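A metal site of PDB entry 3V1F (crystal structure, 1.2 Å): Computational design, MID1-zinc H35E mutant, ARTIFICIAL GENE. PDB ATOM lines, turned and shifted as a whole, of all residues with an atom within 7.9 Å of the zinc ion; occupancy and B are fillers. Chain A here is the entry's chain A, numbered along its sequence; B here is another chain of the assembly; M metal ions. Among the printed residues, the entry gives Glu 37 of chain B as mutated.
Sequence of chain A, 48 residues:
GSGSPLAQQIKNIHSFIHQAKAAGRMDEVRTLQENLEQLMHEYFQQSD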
ATOM      1  N   HIS A  14       2.559  26.253   4.462  1.00  0.00           N
ATOM      2  CA  HIS A  14       2.400  25.589   5.750  1.00  0.00           C
ATOM      3  C   HIS A  14       0.940  25.184   5.988  1.00  0.00           C
ATOM      4  O   HIS A  14       0.637  24.032   6.358  1.00  0.00           O
ATOM      5  CB  HIS A  14       2.943  26.489   6.876  1.00  0.00           C
ATOM      6  CG  HIS A  14       2.535  26.036   8.232  1.00  0.00           C
ATOM      7  ND1 HIS A  14       1.597  26.700   8.991  1.00  0.00           N
ATOM      8  CD2 HIS A  14       2.890  24.935   8.951  1.00  0.00           C
ATOM      9  CE1 HIS A  14       1.407  26.037  10.119  1.00  0.00           C
ATOM     10  NE2 HIS A  14       2.165  24.950  10.117  1.00  0.00           N
ATOM     11  N   SER A  15       0.001  26.112   5.761  1.00  0.00           N
ATOM     12  CA  SER A  15      -1.415  25.803   5.909  1.00  0.00           C
ATOM     13  C   SER A  15      -1.877  24.729   4.901  1.00  0.00           C
ATOM     14  O   SER A  15      -2.618  23.821   5.242  1.00  0.00           O
ATOM     15  CB  SER A  15      -2.257  27.067   5.714  1.00  0.00           C
ATOM     16  OG  SER A  15      -2.028  27.976   6.735  1.00  0.00           O
ATOM     17  N   ILE A  17      -0.253  22.334   3.560  1.00  0.00           N
ATOM     18  CA  ILE A  17       0.231  20.991   3.884  1.00  0.00           C
ATOM     19  C   ILE A  17      -0.732  20.346   4.894  1.00  0.00           C
ATOM     20  O   ILE A  17      -1.108  19.169   4.730  1.00  0.00           O
ATOM     21  CB  ILE A  17       1.676  21.026   4.403  1.00  0.00           C
ATOM     22  CG1 ILE A  17       2.626  21.355   3.259  1.00  0.00           C
ATOM     23  CG2 ILE A  17       2.073  19.685   5.061  1.00  0.00           C
ATOM     24  CD1 ILE A  17       4.034  21.695   3.663  1.00  0.00           C
ATOM     25  N   HIS A  18      -1.158  21.072   5.925  1.00  0.00           N
ATOM     26  CA  HIS A  18      -2.132  20.513   6.867  1.00  0.00           C
ATOM     27  C   HIS A  18      -3.409  20.125   6.126  1.00  0.00           C
ATOM     28  O   HIS A  18      -4.005  19.074   6.393  1.00  0.00           O
ATOM     29  CB  HIS A  18      -2.461  21.499   7.972  1.00  0.00           C
ATOM     30  CG  HIS A  18      -1.372  21.668   8.989  1.00  0.00           C
ATOM     31  ND1 HIS A  18      -0.993  20.651   9.833  1.00  0.00           N
ATOM     32  CD2 HIS A  18      -0.579  22.720   9.283  1.00  0.00           C
ATOM     33  CE1 HIS A  18      -0.032  21.104  10.631  1.00  0.00           C
ATOM     34  NE2 HIS A  18       0.224  22.347  10.328  1.00  0.00           N
ATOM     35  N   LYS A  21      -2.957  16.928   4.040  1.00  0.00           N
ATOM     36  CA  LYS A  21      -2.937  15.745   4.888  1.00  0.00           C
ATOM     37  C   LYS A  21      -4.361  15.386   5.301  1.00  0.00           C
ATOM     38  O   LYS A  21      -4.721  14.195   5.311  1.00  0.00           O
ATOM     39  CB  LYS A  21      -2.068  16.000   6.123  1.00  0.00           C
ATOM     40  CG  LYS A  21      -0.586  15.973   5.843  1.00  0.00           C
ATOM     41  CD  LYS A  21       0.272  16.241   7.076  1.00  0.00           C
ATOM     42  CE  LYS A  21       1.744  16.211   6.706  1.00  0.00           C
ATOM     43  NZ  LYS A  21       2.616  16.584   7.832  1.00  0.00           N
ATOM     44  N   LEU B  36      11.010  21.055  11.301  1.00  0.00           N
ATOM     45  CA  LEU B  36      10.638  22.270  10.597  1.00  0.00           C
ATOM     46  C   LEU B  36       9.180  22.586  10.820  1.00  0.00           C
ATOM     47  O   LEU B  36       8.823  23.746  11.069  1.00  0.00           O
ATOM     48  CB  LEU B  36      10.940  22.112   9.111  1.00  0.00           C
ATOM     49  CG  LEU B  36      10.709  23.330   8.237  1.00  0.00           C
ATOM     50  CD1 LEU B  36      11.622  24.450   8.674  1.00  0.00           C
ATOM     51  CD2 LEU B  36      10.962  22.963   6.803  1.00  0.00           C
ATOM     52  N   GLU B  37       8.324  21.572  10.768  1.00  0.00           N
ATOM     53  CA  GLU B  37       6.906  21.778  11.026  1.00  0.00           C
ATOM     54  C   GLU B  37       6.663  22.288  12.438  1.00  0.00           C
ATOM     55  O   GLU B  37       5.839  23.182  12.646  1.00  0.00           O
ATOM     56  CB  GLU B  37       6.113  20.475  10.790  1.00  0.00           C
ATOM     57  CG  GLU B  37       4.729  20.466  11.419  1.00  0.00           C
ATOM     58  CD  GLU B  37       3.829  21.583  10.975  1.00  0.00           C
ATOM     59  OE1 GLU B  37       3.947  22.103   9.829  1.00  0.00           O
ATOM     60  OE2 GLU B  37       2.966  21.988  11.791  1.00  0.00           O
ATOM     61  N   GLN B  38       7.356  21.724  13.430  1.00  0.00           N
ATOM     62  CA  GLN B  38       7.140  22.200  14.805  1.00  0.00           C
ATOM     63  C   GLN B  38       7.436  23.702  14.906  1.00  0.00           C
ATOM     64  O   GLN B  38       6.701  24.465  15.536  1.00  0.00           O
ATOM     65  CB  GLN B  38       8.011  21.404  15.790  1.00  0.00           C
ATOM     66  CG  GLN B  38       7.763  21.810  17.236  1.00  0.00           C
ATOM     67  CD  GLN B  38       8.556  21.006  18.243  1.00  0.00           C
ATOM     68  OE1 GLN B  38       9.646  20.493  17.957  1.00  0.00           O
ATOM     69  NE2 GLN B  38       8.040  20.929  19.450  1.00  0.00           N
ATOM     70  N   LEU B  39       8.525  24.118  14.276  1.00  0.00           N
ATOM     71  CA  LEU B  39       8.918  25.525  14.273  1.00  0.00           C
ATOM     72  C   LEU B  39       7.970  26.397  13.481  1.00  0.00           C
ATOM     73  O   LEU B  39       7.592  27.473  13.942  1.00  0.00           O
ATOM     74  CB  LEU B  39      10.306  25.672  13.705  1.00  0.00           C
ATOM     75  CG  LEU B  39      11.412  25.086  14.563  1.00  0.00           C
ATOM     76  CD1 LEU B  39      12.634  24.873  13.696  1.00  0.00           C
ATOM     77  CD2 LEU B  39      11.733  25.944  15.779  1.00  0.00           C
ATOM     78  N   MET B  40       7.579  25.971  12.295  1.00  0.00           N
ATOM     79  CA  MET B  40       6.670  26.765  11.467  1.00  0.00           C
ATOM     80  C   MET B  40       5.327  26.936  12.143  1.00  0.00           C
ATOM     81  O   MET B  40       4.730  28.007  12.064  1.00  0.00           O
ATOM     82  CB  MET B  40       6.431  26.111  10.102  1.00  0.00           C
ATOM     83  CG  MET B  40       7.593  26.208   9.144  1.00  0.00           C
ATOM     84  SD  MET B  40       7.175  25.693   7.472  1.00  0.00           S
ATOM     85  CE  MET B  40       6.706  23.978   7.653  1.00  0.00           C
ATOM     86  N   HIS B  41       4.867  25.909  12.821  1.00  0.00           N
ATOM     87  CA  HIS B  41       3.568  25.965  13.445  1.00  0.00           C
ATOM     88  C   HIS B  41       3.581  27.057  14.508  1.00  0.00           C
ATOM     89  O   HIS B  41       2.615  27.786  14.664  1.00  0.00           O
ATOM     90  CB  HIS B  41       3.190  24.626  14.073  1.00  0.00           C
ATOM     91  CG  HIS B  41       1.720  24.418  14.156  1.00  0.00           C
ATOM     92  ND1 HIS B  41       0.979  24.015  13.073  1.00  0.00           N
ATOM     93  CD2 HIS B  41       0.827  24.632  15.159  1.00  0.00           C
ATOM     94  CE1 HIS B  41      -0.297  23.956  13.411  1.00  0.00           C
ATOM     95  NE2 HIS B  41      -0.413  24.330  14.666  1.00  0.00           N
ATOM     96  N   GLU B  42       4.681  27.187  15.237  1.00  0.00           N
ATOM     97  CA  GLU B  42       4.859  28.260  16.227  1.00  0.00           C
ATOM     98  C   GLU B  42       5.074  29.625  15.581  1.00  0.00           C
ATOM     99  O   GLU B  42       4.511  30.632  15.998  1.00  0.00           O
ATOM    100  CB  GLU B  42       6.083  27.923  17.086  1.00  0.00           C
ATOM    101  CG  GLU B  42       5.838  26.755  17.960  1.00  0.00           C
ATOM    102  CD  GLU B  42       7.101  26.110  18.535  1.00  0.00           C
ATOM    103  OE1 GLU B  42       8.248  26.285  18.045  1.00  0.00           O
ATOM    104  OE2 GLU B  42       6.904  25.360  19.505  1.00  0.00           O
ATOM    105  N   PHE B  44       4.238  30.829  12.724  1.00  0.00           N
ATOM    106  CA  PHE B  44       3.144  31.376  11.916  1.00  0.00           C
ATOM    107  C   PHE B  44       1.843  31.529  12.705  1.00  0.00           C
ATOM    108  O   PHE B  44       0.842  31.993  12.161  1.00  0.00           O
ATOM    109  CB  PHE B  44       2.896  30.519  10.666  1.00  0.00           C
ATOM    110  CG  PHE B  44       3.978  30.622   9.655  1.00  0.00           C
ATOM    111  CD1 PHE B  44       4.403  31.871   9.193  1.00  0.00           C
ATOM    112  CD2 PHE B  44       4.531  29.461   9.092  1.00  0.00           C
ATOM    113  CE1 PHE B  44       5.404  31.975   8.244  1.00  0.00           C
ATOM    114  CE2 PHE B  44       5.553  29.555   8.164  1.00  0.00           C
ATOM    115  CZ  PHE B  44       5.966  30.820   7.726  1.00  0.00           C
HETATM  116 ZN    ZN M   1       1.679  23.391  11.263  1.00  0.00          ZN
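OE2 of Glu 37 of chain B is bound to the zinc ion.
NE2 of His 14 is bound to the zinc ion (2.0 Å).
A ring nitrogen (NE2) of His 18 binds the zinc ion (2.0 Å).
ND1 of His 41 of chain B is bound to the zinc ion, 2.0 Å away.
The zinc ion has four donor atoms within binding distance.
Of the 13 residues printed, 4 come within 4 Å of the zinc ion.
The nearest printed residue that does not touch the zinc ion is Met 40 of chain B (5.2 Å).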
